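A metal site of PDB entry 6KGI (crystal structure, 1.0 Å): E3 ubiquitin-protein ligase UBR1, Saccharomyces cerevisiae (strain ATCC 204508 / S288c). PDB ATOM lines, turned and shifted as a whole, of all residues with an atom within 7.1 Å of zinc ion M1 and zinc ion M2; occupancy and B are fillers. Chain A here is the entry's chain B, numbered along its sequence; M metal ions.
The nearest printed residue that does not touch zinc ion M2 is Cys 69 (4.1 Å).
N of Cys 15 is in hydrogen-bond range of ND1 of His 10. The backbone NH (N) of Cys 69 lies close to the side-chain sulfur (SG) of Cys 67 (3.4 Å). The backbone carbonyl oxygen (O) of Cys 43 sits at hydrogen-bond distance from the backbone NH (N) of Lys 82 (3.0 Å). The backbone NH (N) of Cys 15 sits at hydrogen-bond distance from the backbone carbonyl oxygen (O) of Cys 69, 2.8 Å away. A ring nitrogen (ND1) of His 10 is in hydrogen-bond range of the backbone carbonyl oxygen of Arg 13 (2.9 Å). The backbone carbonyl oxygen of Arg 17 is in hydrogen-bond range of the backbone NH of Cys 67. N of His 42 sits close to SG of Cys 40. SG of Cys 15 lies close to N of Arg 17 (3.6 Å).
Zinc ion M2 is bound by the side-chain sulfur (SG) of Cys 67, 2.3 Å away. Zinc ion M2 is bound by the side-chain sulfur (SG) of Cys 40 (2.3 Å). SG of Cys 15 binds zinc ion M2. SG of Cys 43 binds zinc ion M2 (2.4 Å).
Of the 27 residues printed, 4 come within 4 Å of zinc ion M1.
NE2 of His 10 binds zinc ion M1 (2.0 Å). SG of Cys 81 is bound to zinc ion M1 (2.3 Å). Zinc ion M1 is bound by the side-chain sulfur (SG) of Cys 69 (2.3 Å). SG of Cys 43 is bound to zinc ion M1 (2.3 Å).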
ATOM      1  N   HIS A   8     -15.218 -17.518  27.235  1.00  0.00           N
ATOM      2  CA  HIS A   8     -14.923 -18.939  27.313  1.00  0.00           C
ATOM      3  C   HIS A   8     -14.965 -19.615  25.954  1.00  0.00           C
ATOM      4  O   HIS A   8     -14.679 -20.811  25.859  1.00  0.00           O
ATOM      5  CB  HIS A   8     -15.893 -19.637  28.266  1.00  0.00           C
ATOM      6  CG  HIS A   8     -15.908 -19.027  29.632  1.00  0.00           C
ATOM      7  ND1 HIS A   8     -16.877 -18.134  30.027  1.00  0.00           N
ATOM      8  CD2 HIS A   8     -15.063 -19.168  30.671  1.00  0.00           C
ATOM      9  CE1 HIS A   8     -16.625 -17.761  31.273  1.00  0.00           C
ATOM     10  NE2 HIS A   8     -15.539 -18.376  31.687  1.00  0.00           N
ATOM     11  N   LYS A   9     -15.326 -18.889  24.901  1.00  0.00           N
ATOM     12  CA  LYS A   9     -15.316 -19.444  23.562  1.00  0.00           C
ATOM     13  C   LYS A   9     -13.918 -19.936  23.229  1.00  0.00           C
ATOM     14  O   LYS A   9     -12.926 -19.264  23.512  1.00  0.00           O
ATOM     15  CB  LYS A   9     -15.749 -18.366  22.566  1.00  0.00           C
ATOM     16  CG  LYS A   9     -15.699 -18.762  21.102  1.00  0.00           C
ATOM     17  CD  LYS A   9     -16.209 -17.647  20.210  1.00  0.00           C
ATOM     18  CE  LYS A   9     -16.047 -17.959  18.746  1.00  0.00           C
ATOM     19  NZ  LYS A   9     -16.654 -16.904  17.903  1.00  0.00           N
ATOM     20  N   HIS A  10     -13.837 -21.111  22.599  1.00  0.00           N
ATOM     21  CA  HIS A  10     -12.544 -21.705  22.305  1.00  0.00           C
ATOM     22  C   HIS A  10     -12.563 -22.450  20.968  1.00  0.00           C
ATOM     23  O   HIS A  10     -11.820 -23.414  20.776  1.00  0.00           O
ATOM     24  CB  HIS A  10     -12.093 -22.619  23.433  1.00  0.00           C
ATOM     25  CG  HIS A  10     -13.035 -23.759  23.665  1.00  0.00           C
ATOM     26  ND1 HIS A  10     -12.927 -24.953  22.992  1.00  0.00           N
ATOM     27  CD2 HIS A  10     -14.129 -23.875  24.464  1.00  0.00           C
ATOM     28  CE1 HIS A  10     -13.906 -25.768  23.380  1.00  0.00           C
ATOM     29  NE2 HIS A  10     -14.649 -25.131  24.268  1.00  0.00           N
ATOM     30  N   THR A  11     -13.406 -21.991  20.041  1.00  0.00           N
ATOM     31  CA  THR A  11     -13.415 -22.507  18.686  1.00  0.00           C
ATOM     32  C   THR A  11     -11.992 -22.656  18.189  1.00  0.00           C
ATOM     33  O   THR A  11     -11.181 -21.736  18.344  1.00  0.00           O
ATOM     34  CB  THR A  11     -14.161 -21.519  17.792  1.00  0.00           C
ATOM     35  OG1 THR A  11     -15.384 -21.132  18.427  1.00  0.00           O
ATOM     36  CG2 THR A  11     -14.451 -22.110  16.404  1.00  0.00           C
ATOM     37  N   ARG A  13      -9.830 -25.082  19.230  1.00  0.00           N
ATOM     38  CA  ARG A  13      -8.968 -25.770  20.173  1.00  0.00           C
ATOM     39  C   ARG A  13      -9.823 -26.487  21.207  1.00  0.00           C
ATOM     40  O   ARG A  13     -11.042 -26.291  21.290  1.00  0.00           O
ATOM     41  CB  ARG A  13      -8.012 -24.804  20.877  1.00  0.00           C
ATOM     42  CG  ARG A  13      -8.744 -23.765  21.721  1.00  0.00           C
ATOM     43  CD  ARG A  13      -7.775 -22.821  22.388  1.00  0.00           C
ATOM     44  NE  ARG A  13      -8.403 -21.745  23.129  1.00  0.00           N
ATOM     45  CZ  ARG A  13      -8.846 -21.835  24.377  1.00  0.00           C
ATOM     46  NH1 ARG A  13      -8.786 -22.991  25.041  1.00  0.00           N
ATOM     47  NH2 ARG A  13      -9.348 -20.761  24.968  1.00  0.00           N
ATOM     48  N   ASN A  14      -9.161 -27.309  22.025  1.00  0.00           N
ATOM     49  CA  ASN A  14      -9.792 -27.858  23.206  1.00  0.00           C
ATOM     50  C   ASN A  14      -9.956 -26.778  24.271  1.00  0.00           C
ATOM     51  O   ASN A  14      -9.150 -25.848  24.365  1.00  0.00           O
ATOM     52  CB  ASN A  14      -8.935 -28.978  23.791  1.00  0.00           C
ATOM     53  CG  ASN A  14      -7.569 -28.471  24.261  1.00  0.00           C
ATOM     54  OD1 ASN A  14      -6.798 -27.905  23.473  1.00  0.00           O
ATOM     55  ND2 ASN A  14      -7.286 -28.649  25.545  1.00  0.00           N
ATOM     56  N   CYS A  15     -10.989 -26.919  25.099  1.00  0.00           N
ATOM     57  CA  CYS A  15     -11.219 -25.953  26.169  1.00  0.00           C
ATOM     58  C   CYS A  15     -10.059 -25.933  27.162  1.00  0.00           C
ATOM     59  O   CYS A  15      -9.399 -24.899  27.359  1.00  0.00           O
ATOM     60  CB  CYS A  15     -12.525 -26.296  26.899  1.00  0.00           C
ATOM     61  SG  CYS A  15     -12.778 -25.240  28.358  1.00  0.00           S
ATOM     62  N   GLY A  16      -9.789 -27.078  27.782  1.00  0.00           N
ATOM     63  CA  GLY A  16      -8.663 -27.220  28.677  1.00  0.00           C
ATOM     64  C   GLY A  16      -8.777 -26.525  30.004  1.00  0.00           C
ATOM     65  O   GLY A  16      -7.786 -26.476  30.744  1.00  0.00           O
ATOM     66  N   ARG A  17      -9.938 -25.985  30.359  1.00  0.00           N
ATOM     67  CA  ARG A  17     -10.099 -25.313  31.638  1.00  0.00           C
ATOM     68  C   ARG A  17      -9.766 -26.279  32.774  1.00  0.00           C
ATOM     69  O   ARG A  17     -10.276 -27.403  32.813  1.00  0.00           O
ATOM     70  CB  ARG A  17     -11.533 -24.824  31.798  1.00  0.00           C
ATOM     71  CG  ARG A  17     -11.816 -24.113  33.100  1.00  0.00           C
ATOM     72  CD  ARG A  17     -13.295 -23.807  33.236  1.00  0.00           C
ATOM     73  NE  ARG A  17     -13.530 -22.907  34.359  1.00  0.00           N
ATOM     74  CZ  ARG A  17     -13.277 -21.612  34.327  1.00  0.00           C
ATOM     75  NH1 ARG A  17     -12.803 -21.046  33.216  1.00  0.00           N
ATOM     76  NH2 ARG A  17     -13.513 -20.864  35.399  1.00  0.00           N
ATOM     77  N   PHE A  19     -10.186 -27.330  36.567  1.00  0.00           N
ATOM     78  CA  PHE A  19     -11.206 -27.125  37.586  1.00  0.00           C
ATOM     79  C   PHE A  19     -10.583 -26.700  38.907  1.00  0.00           C
ATOM     80  O   PHE A  19      -9.494 -27.153  39.275  1.00  0.00           O
ATOM     81  CB  PHE A  19     -12.003 -28.414  37.773  1.00  0.00           C
ATOM     82  CG  PHE A  19     -12.690 -28.859  36.531  1.00  0.00           C
ATOM     83  CD1 PHE A  19     -13.806 -28.190  36.068  1.00  0.00           C
ATOM     84  CD2 PHE A  19     -12.197 -29.923  35.799  1.00  0.00           C
ATOM     85  CE1 PHE A  19     -14.425 -28.584  34.903  1.00  0.00           C
ATOM     86  CE2 PHE A  19     -12.819 -30.323  34.642  1.00  0.00           C
ATOM     87  CZ  PHE A  19     -13.925 -29.649  34.187  1.00  0.00           C
ATOM     88  N   VAL A  38     -15.271 -35.080  30.639  1.00  0.00           N
ATOM     89  CA  VAL A  38     -16.020 -34.077  31.384  1.00  0.00           C
ATOM     90  C   VAL A  38     -16.130 -32.766  30.622  1.00  0.00           C
ATOM     91  O   VAL A  38     -15.319 -32.454  29.735  1.00  0.00           O
ATOM     92  CB  VAL A  38     -15.404 -33.811  32.778  1.00  0.00           C
ATOM     93  CG1 VAL A  38     -15.438 -35.063  33.635  1.00  0.00           C
ATOM     94  CG2 VAL A  38     -13.968 -33.297  32.635  1.00  0.00           C
ATOM     95  N   LEU A  39     -17.135 -31.988  31.020  1.00  0.00           N
ATOM     96  CA  LEU A  39     -17.400 -30.678  30.448  1.00  0.00           C
ATOM     97  C   LEU A  39     -17.572 -29.650  31.549  1.00  0.00           C
ATOM     98  O   LEU A  39     -18.334 -29.856  32.509  1.00  0.00           O
ATOM     99  CB  LEU A  39     -18.678 -30.707  29.603  1.00  0.00           C
ATOM    100  CG  LEU A  39     -18.613 -31.593  28.360  1.00  0.00           C
ATOM    101  CD1 LEU A  39     -19.997 -31.879  27.803  1.00  0.00           C
ATOM    102  CD2 LEU A  39     -17.728 -30.959  27.300  1.00  0.00           C
ATOM    103  N   CYS A  40     -16.899 -28.511  31.399  1.00  0.00           N
ATOM    104  CA  CYS A  40     -17.054 -27.415  32.346  1.00  0.00           C
ATOM    105  C   CYS A  40     -18.402 -26.737  32.145  1.00  0.00           C
ATOM    106  O   CYS A  40     -19.105 -26.953  31.163  1.00  0.00           O
ATOM    107  CB  CYS A  40     -15.901 -26.419  32.203  1.00  0.00           C
ATOM    108  SG  CYS A  40     -16.024 -25.276  30.796  1.00  0.00           S
ATOM    109  N   ILE A  41     -18.771 -25.916  33.132  1.00  0.00           N
ATOM    110  CA  ILE A  41     -20.085 -25.284  33.118  1.00  0.00           C
ATOM    111  C   ILE A  41     -20.233 -24.314  31.950  1.00  0.00           C
ATOM    112  O   ILE A  41     -21.345 -24.030  31.524  1.00  0.00           O
ATOM    113  CB  ILE A  41     -20.379 -24.581  34.463  1.00  0.00           C
ATOM    114  CG1 ILE A  41     -19.379 -23.453  34.729  1.00  0.00           C
ATOM    115  CG2 ILE A  41     -20.426 -25.582  35.585  1.00  0.00           C
ATOM    116  CD1 ILE A  41     -19.634 -22.686  36.006  1.00  0.00           C
ATOM    117  N   HIS A  42     -19.129 -23.744  31.462  1.00  0.00           N
ATOM    118  CA  HIS A  42     -19.192 -22.787  30.370  1.00  0.00           C
ATOM    119  C   HIS A  42     -19.395 -23.467  29.026  1.00  0.00           C
ATOM    120  O   HIS A  42     -19.847 -22.826  28.070  1.00  0.00           O
ATOM    121  CB  HIS A  42     -17.923 -21.941  30.365  1.00  0.00           C
ATOM    122  CG  HIS A  42     -17.604 -21.398  31.714  1.00  0.00           C
ATOM    123  ND1 HIS A  42     -18.379 -20.427  32.306  1.00  0.00           N
ATOM    124  CD2 HIS A  42     -16.657 -21.738  32.613  1.00  0.00           C
ATOM    125  CE1 HIS A  42     -17.893 -20.173  33.512  1.00  0.00           C
ATOM    126  NE2 HIS A  42     -16.853 -20.959  33.724  1.00  0.00           N
ATOM    127  N   CYS A  43     -19.067 -24.744  28.950  1.00  0.00           N
ATOM    128  CA  CYS A  43     -19.105 -25.517  27.715  1.00  0.00           C
ATOM    129  C   CYS A  43     -20.320 -26.417  27.608  1.00  0.00           C
ATOM    130  O   CYS A  43     -20.861 -26.582  26.502  1.00  0.00           O
ATOM    131  CB  CYS A  43     -17.852 -26.394  27.624  1.00  0.00           C
ATOM    132  SG  CYS A  43     -16.375 -25.435  27.298  1.00  0.00           S
ATOM    133  N   PHE A  44     -20.741 -27.040  28.707  1.00  0.00           N
ATOM    134  CA  PHE A  44     -21.830 -27.993  28.645  1.00  0.00           C
ATOM    135  C   PHE A  44     -23.064 -27.342  28.032  1.00  0.00           C
ATOM    136  O   PHE A  44     -23.531 -26.311  28.512  1.00  0.00           O
ATOM    137  CB  PHE A  44     -22.185 -28.490  30.050  1.00  0.00           C
ATOM    138  CG  PHE A  44     -23.363 -29.436  30.065  1.00  0.00           C
ATOM    139  CD1 PHE A  44     -23.187 -30.785  29.798  1.00  0.00           C
ATOM    140  CD2 PHE A  44     -24.637 -28.974  30.331  1.00  0.00           C
ATOM    141  CE1 PHE A  44     -24.271 -31.662  29.783  1.00  0.00           C
ATOM    142  CE2 PHE A  44     -25.720 -29.843  30.322  1.00  0.00           C
ATOM    143  CZ  PHE A  44     -25.532 -31.188  30.050  1.00  0.00           C
ATOM    144  N   ILE A  66      -9.133 -31.451  33.570  1.00  0.00           N
ATOM    145  CA  ILE A  66      -9.470 -30.364  32.670  1.00  0.00           C
ATOM    146  C   ILE A  66     -10.705 -30.699  31.857  1.00  0.00           C
ATOM    147  O   ILE A  66     -11.045 -31.861  31.643  1.00  0.00           O
ATOM    148  CB  ILE A  66      -8.301 -30.005  31.717  1.00  0.00           C
ATOM    149  CG1 ILE A  66      -8.001 -31.165  30.762  1.00  0.00           C
ATOM    150  CG2 ILE A  66      -7.054 -29.632  32.513  1.00  0.00           C
ATOM    151  CD1 ILE A  66      -6.879 -30.865  29.773  1.00  0.00           C
ATOM    152  N   CYS A  67     -11.356 -29.647  31.363  1.00  0.00           N
ATOM    153  CA  CYS A  67     -12.517 -29.795  30.484  1.00  0.00           C
ATOM    154  C   CYS A  67     -12.095 -30.354  29.126  1.00  0.00           C
ATOM    155  O   CYS A  67     -11.137 -29.866  28.508  1.00  0.00           O
ATOM    156  CB  CYS A  67     -13.161 -28.430  30.271  1.00  0.00           C
ATOM    157  SG  CYS A  67     -14.547 -28.435  29.126  1.00  0.00           S
ATOM    158  N   ASP A  68     -12.863 -31.333  28.654  1.00  0.00           N
ATOM    159  CA  ASP A  68     -12.584 -32.016  27.398  1.00  0.00           C
ATOM    160  C   ASP A  68     -13.396 -31.482  26.211  1.00  0.00           C
ATOM    161  O   ASP A  68     -13.358 -32.089  25.132  1.00  0.00           O
ATOM    162  CB  ASP A  68     -12.862 -33.513  27.543  1.00  0.00           C
ATOM    163  CG  ASP A  68     -12.019 -34.169  28.608  1.00  0.00           C
ATOM    164  OD1 ASP A  68     -10.762 -34.153  28.464  1.00  0.00           O
ATOM    165  OD2 ASP A  68     -12.593 -34.702  29.586  1.00  0.00           O
ATOM    166  N   CYS A  69     -14.124 -30.379  26.371  1.00  0.00           N
ATOM    167  CA  CYS A  69     -14.860 -29.821  25.246  1.00  0.00           C
ATOM    168  C   CYS A  69     -13.890 -29.500  24.110  1.00  0.00           C
ATOM    169  O   CYS A  69     -12.841 -28.914  24.336  1.00  0.00           O
ATOM    170  CB  CYS A  69     -15.595 -28.553  25.699  1.00  0.00           C
ATOM    171  SG  CYS A  69     -16.770 -27.934  24.441  1.00  0.00           S
ATOM    172  N   GLY A  70     -14.221 -29.917  22.892  1.00  0.00           N
ATOM    173  CA  GLY A  70     -13.352 -29.666  21.770  1.00  0.00           C
ATOM    174  C   GLY A  70     -12.288 -30.724  21.548  1.00  0.00           C
ATOM    175  O   GLY A  70     -11.512 -30.603  20.581  1.00  0.00           O
ATOM    176  N   HIS A  80     -21.730 -29.047  20.721  1.00  0.00           N
ATOM    177  CA  HIS A  80     -21.901 -27.659  20.271  1.00  0.00           C
ATOM    178  C   HIS A  80     -21.685 -26.798  21.496  1.00  0.00           C
ATOM    179  O   HIS A  80     -22.602 -26.583  22.285  1.00  0.00           O
ATOM    180  CB  HIS A  80     -23.265 -27.499  19.629  1.00  0.00           C
ATOM    181  CG  HIS A  80     -23.491 -28.476  18.535  1.00  0.00           C
ATOM    182  ND1 HIS A  80     -23.912 -29.760  18.775  1.00  0.00           N
ATOM    183  CD2 HIS A  80     -23.300 -28.387  17.191  1.00  0.00           C
ATOM    184  CE1 HIS A  80     -24.008 -30.423  17.630  1.00  0.00           C
ATOM    185  NE2 HIS A  80     -23.636 -29.615  16.653  1.00  0.00           N
ATOM    186  N   CYS A  81     -20.448 -26.329  21.650  1.00  0.00           N
ATOM    187  CA  CYS A  81     -20.051 -25.642  22.876  1.00  0.00           C
ATOM    188  C   CYS A  81     -21.007 -24.510  23.208  1.00  0.00           C
ATOM    189  O   CYS A  81     -21.303 -23.661  22.366  1.00  0.00           O
ATOM    190  CB  CYS A  81     -18.637 -25.103  22.718  1.00  0.00           C
ATOM    191  SG  CYS A  81     -18.043 -24.232  24.185  1.00  0.00           S
ATOM    192  N   LYS A  82     -21.468 -24.479  24.464  1.00  0.00           N
ATOM    193  CA  LYS A  82     -22.391 -23.421  24.857  1.00  0.00           C
ATOM    194  C   LYS A  82     -21.756 -22.040  24.692  1.00  0.00           C
ATOM    195  O   LYS A  82     -22.448 -21.072  24.355  1.00  0.00           O
ATOM    196  CB  LYS A  82     -22.829 -23.630  26.305  1.00  0.00           C
ATOM    197  CG  LYS A  82     -23.948 -22.692  26.716  1.00  0.00           C
ATOM    198  CD  LYS A  82     -24.421 -22.955  28.123  1.00  0.00           C
ATOM    199  CE  LYS A  82     -23.375 -22.498  29.116  1.00  0.00           C
ATOM    200  NZ  LYS A  82     -23.925 -22.469  30.494  1.00  0.00           N
ATOM    201  N   ALA A  83     -20.441 -21.935  24.901  1.00  0.00           N
ATOM    202  CA  ALA A  83     -19.770 -20.651  24.808  1.00  0.00           C
ATOM    203  C   ALA A  83     -19.656 -20.128  23.385  1.00  0.00           C
ATOM    204  O   ALA A  83     -19.313 -18.950  23.205  1.00  0.00           O
ATOM    205  CB  ALA A  83     -18.377 -20.746  25.431  1.00  0.00           C
ATOM    206  N   GLU A  84     -19.914 -20.963  22.388  1.00  0.00           N
ATOM    207  CA  GLU A  84     -19.939 -20.506  21.007  1.00  0.00           C
ATOM    208  C   GLU A  84     -21.289 -19.919  20.630  1.00  0.00           C
ATOM    209  O   GLU A  84     -21.369 -19.180  19.640  1.00  0.00           O
ATOM    210  CB  GLU A  84     -19.650 -21.689  20.082  1.00  0.00           C
ATOM    211  CG  GLU A  84     -18.751 -21.391  18.915  1.00  0.00           C
ATOM    212  CD  GLU A  84     -18.381 -22.637  18.130  1.00  0.00           C
ATOM    213  OE1 GLU A  84     -19.182 -23.043  17.268  1.00  0.00           O
ATOM    214  OE2 GLU A  84     -17.289 -23.198  18.376  1.00  0.00           O
HETATM  215 ZN    ZN M   1     -16.468 -25.706  24.968  1.00  0.00          ZN
HETATM  216 ZN    ZN M   2     -14.848 -26.136  28.981  1.00  0.00          ZN
